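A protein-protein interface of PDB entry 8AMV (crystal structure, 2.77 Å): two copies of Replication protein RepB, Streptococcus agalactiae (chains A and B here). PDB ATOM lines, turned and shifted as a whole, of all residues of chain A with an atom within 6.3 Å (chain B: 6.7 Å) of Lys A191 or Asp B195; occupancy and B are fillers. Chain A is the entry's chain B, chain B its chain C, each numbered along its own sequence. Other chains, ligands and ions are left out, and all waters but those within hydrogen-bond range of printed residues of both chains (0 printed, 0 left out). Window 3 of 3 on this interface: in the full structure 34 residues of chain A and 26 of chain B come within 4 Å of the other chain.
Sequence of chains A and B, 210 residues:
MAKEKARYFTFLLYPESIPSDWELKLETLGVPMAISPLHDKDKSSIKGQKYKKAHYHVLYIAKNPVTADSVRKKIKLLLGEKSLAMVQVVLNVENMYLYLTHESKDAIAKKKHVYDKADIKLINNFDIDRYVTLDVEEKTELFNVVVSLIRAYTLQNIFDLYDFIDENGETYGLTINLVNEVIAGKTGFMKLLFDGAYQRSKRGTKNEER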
ATOM      1  N   ASN A 157      -6.775 -11.465  -0.762  1.00  0.00           N
ATOM      2  CA  ASN A 157      -7.410 -12.128   0.371  1.00  0.00           C
ATOM      3  C   ASN A 157      -8.154 -13.342  -0.151  1.00  0.00           C
ATOM      4  O   ASN A 157      -8.089 -13.666  -1.338  1.00  0.00           O
ATOM      5  CB  ASN A 157      -8.341 -11.190   1.132  1.00  0.00           C
ATOM      6  CG  ASN A 157      -9.434 -10.654   0.274  1.00  0.00           C
ATOM      7  OD1 ASN A 157     -10.211 -11.401  -0.321  1.00  0.00           O
ATOM      8  ND2 ASN A 157      -9.494  -9.334   0.182  1.00  0.00           N
ATOM      9  N   LYS A 186      -2.658 -24.998   6.040  1.00  0.00           N
ATOM     10  CA  LYS A 186      -1.633 -24.146   5.464  1.00  0.00           C
ATOM     11  C   LYS A 186      -2.005 -22.675   5.616  1.00  0.00           C
ATOM     12  O   LYS A 186      -1.542 -21.828   4.827  1.00  0.00           O
ATOM     13  CB  LYS A 186      -1.400 -24.532   4.006  1.00  0.00           C
ATOM     14  CG  LYS A 186      -0.870 -25.956   3.895  1.00  0.00           C
ATOM     15  CD  LYS A 186      -0.084 -26.236   2.631  1.00  0.00           C
ATOM     16  CE  LYS A 186       1.256 -25.525   2.626  1.00  0.00           C
ATOM     17  NZ  LYS A 186       2.408 -26.470   2.736  1.00  0.00           N
ATOM     18  N   THR A 187      -2.814 -22.341   6.632  1.00  0.00           N
ATOM     19  CA  THR A 187      -3.324 -20.981   6.684  1.00  0.00           C
ATOM     20  C   THR A 187      -2.225 -19.987   6.984  1.00  0.00           C
ATOM     21  O   THR A 187      -2.294 -18.854   6.527  1.00  0.00           O
ATOM     22  CB  THR A 187      -4.449 -20.879   7.689  1.00  0.00           C
ATOM     23  OG1 THR A 187      -3.996 -21.394   8.935  1.00  0.00           O
ATOM     24  CG2 THR A 187      -5.594 -21.697   7.211  1.00  0.00           C
ATOM     25  N   GLY A 188      -1.197 -20.387   7.722  1.00  0.00           N
ATOM     26  CA  GLY A 188      -0.065 -19.491   7.925  1.00  0.00           C
ATOM     27  C   GLY A 188       0.611 -19.129   6.614  1.00  0.00           C
ATOM     28  O   GLY A 188       0.956 -17.968   6.385  1.00  0.00           O
ATOM     29  N   PHE A 189       0.776 -20.116   5.722  1.00  0.00           N
ATOM     30  CA  PHE A 189       1.290 -19.852   4.386  1.00  0.00           C
ATOM     31  C   PHE A 189       0.335 -18.946   3.614  1.00  0.00           C
ATOM     32  O   PHE A 189       0.769 -18.006   2.938  1.00  0.00           O
ATOM     33  CB  PHE A 189       1.513 -21.169   3.637  1.00  0.00           C
ATOM     34  CG  PHE A 189       2.653 -21.140   2.652  1.00  0.00           C
ATOM     35  CD1 PHE A 189       2.732 -20.156   1.645  1.00  0.00           C
ATOM     36  CD2 PHE A 189       3.648 -22.117   2.706  1.00  0.00           C
ATOM     37  CE1 PHE A 189       3.820 -20.155   0.717  1.00  0.00           C
ATOM     38  CE2 PHE A 189       4.728 -22.112   1.801  1.00  0.00           C
ATOM     39  CZ  PHE A 189       4.813 -21.131   0.809  1.00  0.00           C
ATOM     40  N   MET A 190      -0.967 -19.219   3.686  1.00  0.00           N
ATOM     41  CA  MET A 190      -1.948 -18.348   3.039  1.00  0.00           C
ATOM     42  C   MET A 190      -1.788 -16.903   3.500  1.00  0.00           C
ATOM     43  O   MET A 190      -1.781 -15.971   2.689  1.00  0.00           O
ATOM     44  CB  MET A 190      -3.356 -18.839   3.351  1.00  0.00           C
ATOM     45  CG  MET A 190      -3.704 -20.108   2.660  1.00  0.00           C
ATOM     46  SD  MET A 190      -3.766 -19.846   0.893  1.00  0.00           S
ATOM     47  CE  MET A 190      -2.374 -20.817   0.432  1.00  0.00           C
ATOM     48  N   LYS A 191      -1.628 -16.700   4.804  1.00  0.00           N
ATOM     49  CA  LYS A 191      -1.522 -15.349   5.317  1.00  0.00           C
ATOM     50  C   LYS A 191      -0.341 -14.646   4.657  1.00  0.00           C
ATOM     51  O   LYS A 191      -0.467 -13.519   4.180  1.00  0.00           O
ATOM     52  CB  LYS A 191      -1.399 -15.399   6.843  1.00  0.00           C
ATOM     53  CG  LYS A 191      -1.374 -14.054   7.563  1.00  0.00           C
ATOM     54  CD  LYS A 191      -2.511 -13.157   7.134  1.00  0.00           C
ATOM     55  CE  LYS A 191      -2.332 -11.752   7.711  1.00  0.00           C
ATOM     56  NZ  LYS A 191      -3.533 -10.858   7.519  1.00  0.00           N
ATOM     57  N   LEU A 192       0.792 -15.344   4.529  1.00  0.00           N
ATOM     58  CA  LEU A 192       1.958 -14.745   3.901  1.00  0.00           C
ATOM     59  C   LEU A 192       1.646 -14.301   2.481  1.00  0.00           C
ATOM     60  O   LEU A 192       2.069 -13.219   2.061  1.00  0.00           O
ATOM     61  CB  LEU A 192       3.119 -15.735   3.880  1.00  0.00           C
ATOM     62  CG  LEU A 192       3.740 -16.099   5.209  1.00  0.00           C
ATOM     63  CD1 LEU A 192       4.801 -17.113   4.919  1.00  0.00           C
ATOM     64  CD2 LEU A 192       4.328 -14.894   5.894  1.00  0.00           C
ATOM     65  N   LEU A 193       0.940 -15.147   1.717  1.00  0.00           N
ATOM     66  CA  LEU A 193       0.646 -14.861   0.313  1.00  0.00           C
ATOM     67  C   LEU A 193      -0.253 -13.643   0.180  1.00  0.00           C
ATOM     68  O   LEU A 193      -0.038 -12.803  -0.688  1.00  0.00           O
ATOM     69  CB  LEU A 193      -0.005 -16.069  -0.337  1.00  0.00           C
ATOM     70  CG  LEU A 193       0.846 -17.308  -0.521  1.00  0.00           C
ATOM     71  CD1 LEU A 193      -0.070 -18.424  -0.969  1.00  0.00           C
ATOM     72  CD2 LEU A 193       1.973 -17.098  -1.526  1.00  0.00           C
ATOM     73  N   PHE A 194      -1.323 -13.578   0.977  1.00  0.00           N
ATOM     74  CA  PHE A 194      -2.216 -12.425   0.912  1.00  0.00           C
ATOM     75  C   PHE A 194      -1.523 -11.164   1.390  1.00  0.00           C
ATOM     76  O   PHE A 194      -1.781 -10.076   0.861  1.00  0.00           O
ATOM     77  CB  PHE A 194      -3.485 -12.667   1.722  1.00  0.00           C
ATOM     78  CG  PHE A 194      -4.296 -13.796   1.207  1.00  0.00           C
ATOM     79  CD1 PHE A 194      -4.379 -14.025  -0.157  1.00  0.00           C
ATOM     80  CD2 PHE A 194      -4.940 -14.661   2.078  1.00  0.00           C
ATOM     81  CE1 PHE A 194      -5.109 -15.079  -0.653  1.00  0.00           C
ATOM     82  CE2 PHE A 194      -5.661 -15.726   1.589  1.00  0.00           C
ATOM     83  CZ  PHE A 194      -5.753 -15.936   0.224  1.00  0.00           C
ATOM     84  N   ASP A 195      -0.683 -11.265   2.422  1.00  0.00           N
ATOM     85  CA  ASP A 195       0.054 -10.083   2.840  1.00  0.00           C
ATOM     86  C   ASP A 195       0.890  -9.568   1.687  1.00  0.00           C
ATOM     87  O   ASP A 195       0.930  -8.367   1.424  1.00  0.00           O
ATOM     88  CB  ASP A 195       0.946 -10.385   4.041  1.00  0.00           C
ATOM     89  CG  ASP A 195       0.217 -10.255   5.347  1.00  0.00           C
ATOM     90  OD1 ASP A 195      -1.019 -10.079   5.308  1.00  0.00           O
ATOM     91  OD2 ASP A 195       0.880 -10.310   6.413  1.00  0.00           O
ATOM     92  N   GLY A 196       1.589 -10.481   1.009  1.00  0.00           N
ATOM     93  CA  GLY A 196       2.387 -10.127  -0.153  1.00  0.00           C
ATOM     94  C   GLY A 196       1.582  -9.445  -1.234  1.00  0.00           C
ATOM     95  O   GLY A 196       1.996  -8.428  -1.790  1.00  0.00           O
ATOM     96  N   LEU B 155     -19.706 -11.500   6.389  1.00  0.00           N
ATOM     97  CA  LEU B 155     -19.679 -11.532   7.849  1.00  0.00           C
ATOM     98  C   LEU B 155     -18.271 -11.248   8.373  1.00  0.00           C
ATOM     99  O   LEU B 155     -17.366 -12.075   8.222  1.00  0.00           O
ATOM    100  CB  LEU B 155     -20.163 -12.887   8.343  1.00  0.00           C
ATOM    101  CG  LEU B 155     -21.587 -13.199   7.920  1.00  0.00           C
ATOM    102  CD1 LEU B 155     -21.951 -14.607   8.340  1.00  0.00           C
ATOM    103  CD2 LEU B 155     -22.496 -12.189   8.563  1.00  0.00           C
ATOM    104  N   GLN B 156     -18.114 -10.118   9.064  1.00  0.00           N
ATOM    105  CA  GLN B 156     -16.813  -9.515   9.330  1.00  0.00           C
ATOM    106  C   GLN B 156     -16.097 -10.095  10.546  1.00  0.00           C
ATOM    107  O   GLN B 156     -14.905  -9.818  10.732  1.00  0.00           O
ATOM    108  CB  GLN B 156     -16.972  -8.003   9.498  1.00  0.00           C
ATOM    109  CG  GLN B 156     -17.292  -7.283   8.190  1.00  0.00           C
ATOM    110  CD  GLN B 156     -17.526  -5.799   8.377  1.00  0.00           C
ATOM    111  OE1 GLN B 156     -16.611  -5.042   8.703  1.00  0.00           O
ATOM    112  NE2 GLN B 156     -18.771  -5.379   8.192  1.00  0.00           N
ATOM    113  N   MET B 190     -10.643 -19.426   9.881  1.00  0.00           N
ATOM    114  CA  MET B 190     -11.646 -18.436  10.274  1.00  0.00           C
ATOM    115  C   MET B 190     -11.084 -17.025  10.177  1.00  0.00           C
ATOM    116  O   MET B 190     -11.812 -16.088   9.833  1.00  0.00           O
ATOM    117  CB  MET B 190     -12.149 -18.699  11.684  1.00  0.00           C
ATOM    118  CG  MET B 190     -13.018 -19.954  11.798  1.00  0.00           C
ATOM    119  SD  MET B 190     -14.677 -19.848  11.089  1.00  0.00           S
ATOM    120  CE  MET B 190     -14.450 -20.606   9.500  1.00  0.00           C
ATOM    121  N   LYS B 191      -9.819 -16.829  10.578  1.00  0.00           N
ATOM    122  CA  LYS B 191      -9.248 -15.488  10.510  1.00  0.00           C
ATOM    123  C   LYS B 191      -9.160 -15.012   9.065  1.00  0.00           C
ATOM    124  O   LYS B 191      -9.514 -13.868   8.761  1.00  0.00           O
ATOM    125  CB  LYS B 191      -7.882 -15.459  11.187  1.00  0.00           C
ATOM    126  CG  LYS B 191      -7.284 -14.055  11.313  1.00  0.00           C
ATOM    127  CD  LYS B 191      -8.347 -13.034  11.673  1.00  0.00           C
ATOM    128  CE  LYS B 191      -7.735 -11.700  12.015  1.00  0.00           C
ATOM    129  NZ  LYS B 191      -8.598 -10.970  12.991  1.00  0.00           N
ATOM    130  N   LEU B 192      -8.713 -15.886   8.151  1.00  0.00           N
ATOM    131  CA  LEU B 192      -8.628 -15.519   6.738  1.00  0.00           C
ATOM    132  C   LEU B 192      -9.996 -15.092   6.198  1.00  0.00           C
ATOM    133  O   LEU B 192     -10.092 -14.150   5.406  1.00  0.00           O
ATOM    134  CB  LEU B 192      -8.079 -16.685   5.913  1.00  0.00           C
ATOM    135  CG  LEU B 192      -6.637 -17.161   6.069  1.00  0.00           C
ATOM    136  CD1 LEU B 192      -6.447 -18.426   5.269  1.00  0.00           C
ATOM    137  CD2 LEU B 192      -5.525 -16.120   5.731  1.00  0.00           C
ATOM    138  N   LEU B 193     -11.064 -15.815   6.553  1.00  0.00           N
ATOM    139  CA  LEU B 193     -12.382 -15.452   6.038  1.00  0.00           C
ATOM    140  C   LEU B 193     -12.798 -14.091   6.570  1.00  0.00           C
ATOM    141  O   LEU B 193     -13.135 -13.189   5.798  1.00  0.00           O
ATOM    142  CB  LEU B 193     -13.398 -16.512   6.418  1.00  0.00           C
ATOM    143  CG  LEU B 193     -13.202 -17.858   5.736  1.00  0.00           C
ATOM    144  CD1 LEU B 193     -13.961 -18.877   6.514  1.00  0.00           C
ATOM    145  CD2 LEU B 193     -13.634 -17.869   4.289  1.00  0.00           C
ATOM    146  N   PHE B 194     -12.701 -13.899   7.891  1.00  0.00           N
ATOM    147  CA  PHE B 194     -13.083 -12.619   8.483  1.00  0.00           C
ATOM    148  C   PHE B 194     -12.213 -11.493   7.952  1.00  0.00           C
ATOM    149  O   PHE B 194     -12.703 -10.384   7.746  1.00  0.00           O
ATOM    150  CB  PHE B 194     -12.990 -12.665  10.008  1.00  0.00           C
ATOM    151  CG  PHE B 194     -13.997 -13.574  10.656  1.00  0.00           C
ATOM    152  CD1 PHE B 194     -15.244 -13.778  10.086  1.00  0.00           C
ATOM    153  CD2 PHE B 194     -13.693 -14.236  11.838  1.00  0.00           C
ATOM    154  CE1 PHE B 194     -16.158 -14.622  10.674  1.00  0.00           C
ATOM    155  CE2 PHE B 194     -14.608 -15.081  12.432  1.00  0.00           C
ATOM    156  CZ  PHE B 194     -15.838 -15.274  11.841  1.00  0.00           C
ATOM    157  N   ASP B 195     -10.912 -11.743   7.747  1.00  0.00           N
ATOM    158  CA  ASP B 195     -10.055 -10.720   7.147  1.00  0.00           C
ATOM    159  C   ASP B 195     -10.559 -10.342   5.756  1.00  0.00           C
ATOM    160  O   ASP B 195     -10.652  -9.152   5.416  1.00  0.00           O
ATOM    161  CB  ASP B 195      -8.615 -11.219   7.046  1.00  0.00           C
ATOM    162  CG  ASP B 195      -7.777 -10.881   8.276  1.00  0.00           C
ATOM    163  OD1 ASP B 195      -8.324 -10.295   9.239  1.00  0.00           O
ATOM    164  OD2 ASP B 195      -6.561 -11.189   8.275  1.00  0.00           O
ATOM    165  N   GLY B 196     -10.837 -11.359   4.925  1.00  0.00           N
ATOM    166  CA  GLY B 196     -11.431 -11.128   3.615  1.00  0.00           C
ATOM    167  C   GLY B 196     -12.746 -10.375   3.683  1.00  0.00           C
ATOM    168  O   GLY B 196     -12.974  -9.434   2.922  1.00  0.00           O
ATOM    169  N   ALA B 197     -13.661 -10.825   4.539  1.00  0.00           N
ATOM    170  CA  ALA B 197     -14.926 -10.114   4.660  1.00  0.00           C
ATOM    171  C   ALA B 197     -14.666  -8.660   5.020  1.00  0.00           C
ATOM    172  O   ALA B 197     -15.246  -7.738   4.429  1.00  0.00           O
ATOM    173  CB  ALA B 197     -15.813 -10.777   5.710  1.00  0.00           C
ATOM    174  N   TYR B 198     -13.755  -8.433   5.966  1.00  0.00           N
ATOM    175  CA  TYR B 198     -13.494  -7.081   6.437  1.00  0.00           C
ATOM    176  C   TYR B 198     -13.054  -6.193   5.279  1.00  0.00           C
ATOM    177  O   TYR B 198     -13.618  -5.116   5.069  1.00  0.00           O
ATOM    178  CB  TYR B 198     -12.472  -7.116   7.570  1.00  0.00           C
ATOM    179  CG  TYR B 198     -12.269  -5.808   8.295  1.00  0.00           C
ATOM    180  CD1 TYR B 198     -13.229  -5.304   9.164  1.00  0.00           C
ATOM    181  CD2 TYR B 198     -11.105  -5.101   8.157  1.00  0.00           C
ATOM    182  CE1 TYR B 198     -13.031  -4.101   9.846  1.00  0.00           C
ATOM    183  CE2 TYR B 198     -10.893  -3.929   8.849  1.00  0.00           C
ATOM    184  CZ  TYR B 198     -11.854  -3.420   9.664  1.00  0.00           C
ATOM    185  OH  TYR B 198     -11.610  -2.236  10.320  1.00  0.00           O
ATOM    186  N   GLN B 199     -12.067  -6.643   4.492  1.00  0.00           N
ATOM    187  CA  GLN B 199     -11.616  -5.855   3.344  1.00  0.00           C
ATOM    188  C   GLN B 199     -12.759  -5.634   2.361  1.00  0.00           C
ATOM    189  O   GLN B 199     -12.869  -4.564   1.750  1.00  0.00           O
ATOM    190  CB  GLN B 199     -10.493  -6.579   2.611  1.00  0.00           C
ATOM    191  CG  GLN B 199      -9.292  -6.927   3.432  1.00  0.00           C
ATOM    192  CD  GLN B 199      -8.139  -7.438   2.571  1.00  0.00           C
ATOM    193  OE1 GLN B 199      -8.200  -7.427   1.337  1.00  0.00           O
ATOM    194  NE2 GLN B 199      -7.074  -7.892   3.234  1.00  0.00           N
ATOM    195  N   ARG B 200     -13.623  -6.642   2.196  1.00  0.00           N
ATOM    196  CA  ARG B 200     -14.706  -6.546   1.225  1.00  0.00           C
ATOM    197  C   ARG B 200     -15.717  -5.499   1.649  1.00  0.00           C
ATOM    198  O   ARG B 200     -16.283  -4.795   0.808  1.00  0.00           O
ATOM    199  CB  ARG B 200     -15.396  -7.896   1.096  1.00  0.00           C
ATOM    200  CG  ARG B 200     -16.098  -8.100  -0.192  1.00  0.00           C
ATOM    201  CD  ARG B 200     -15.273  -7.562  -1.331  1.00  0.00           C
ATOM    202  NE  ARG B 200     -14.366  -8.545  -1.922  1.00  0.00           N
ATOM    203  CZ  ARG B 200     -14.728  -9.593  -2.662  1.00  0.00           C
ATOM    204  NH1 ARG B 200     -16.004  -9.943  -2.783  1.00  0.00           N
ATOM    205  NH2 ARG B 200     -13.784 -10.376  -3.169  1.00  0.00           N
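NZ of Lys B191 lies within salt-bridge range of OD1 of Asp B195, at 3.8 Å.
OD1 of Asp A195 is in salt-bridge range of NZ of Lys A191, 3.4 Å away.
Gly B196 touches Asn A157 (CA to CG, 3.9 Å).
Thr A187 touches Leu B192.
Leu B192 touches Met A190 (CD1 to CB, 3.7 Å).
Phe A194 touches Leu B192 (CD2 to CD2, 3.98 Å).
Hydrophobic or aromatic side chains of chain A within 4 Å of the printed part of chain B: Met A190 and Phe A194.
Hydrophobic or aromatic side chains of chain B that line the printed part of chain A: Leu B192.
Along chain B the printed residues that touch a printed residue of chain A span positions 192 to 199.
Among the printed residues, 6 pairs touch across the chains.
The side-chain amide nitrogen (ND2) of Asn A157 sits at hydrogen-bond distance from the side-chain amide oxygen (OE1) of Gln B199.
The side-chain amino group (NZ) of Lys A191 is in salt-bridge range of the side-chain carboxylate (OD2) of Asp B195.
Met A190 touches Leu B192, but with the chains exchanged Leu A192 does not touch Met B190 (13.3 Å).
Lys A191 touches Asp B195, but with the chains exchanged Asp A195 does not touch Lys B191 (9.5 Å).
Phe A194 touches Leu B192, but with the chains exchanged Leu A192 does not touch Phe B194 (14.0 Å).
Positions printed for both chains: 190, 191, 192, 193, 194, 195 and 196.
Of the 6 pairs that touch across the chains among the printed residues, none has its exchanged pair printed and touching as well.
Of the printed residues of chain B, Asn A157 touches Gly B196 (3.9 Å) and Gln B199 (2.6 Å).
Of the printed residues of chain B, Met A190 touches Leu B192 (3.7 Å).
Lys A191 touches just one residue of chain B: Asp B195.
Gln B156 touches none of the printed residues of chain A.
Of the printed residues of chain A, Gly B196 touches Asn A157 (3.9 Å).
The nearest residue of chain A that does not touch Asp B195 is Asn A157 (5.2 Å).
The nearest printed residue of chain A that does not touch Leu B192 is Lys A191 (4.05 Å).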
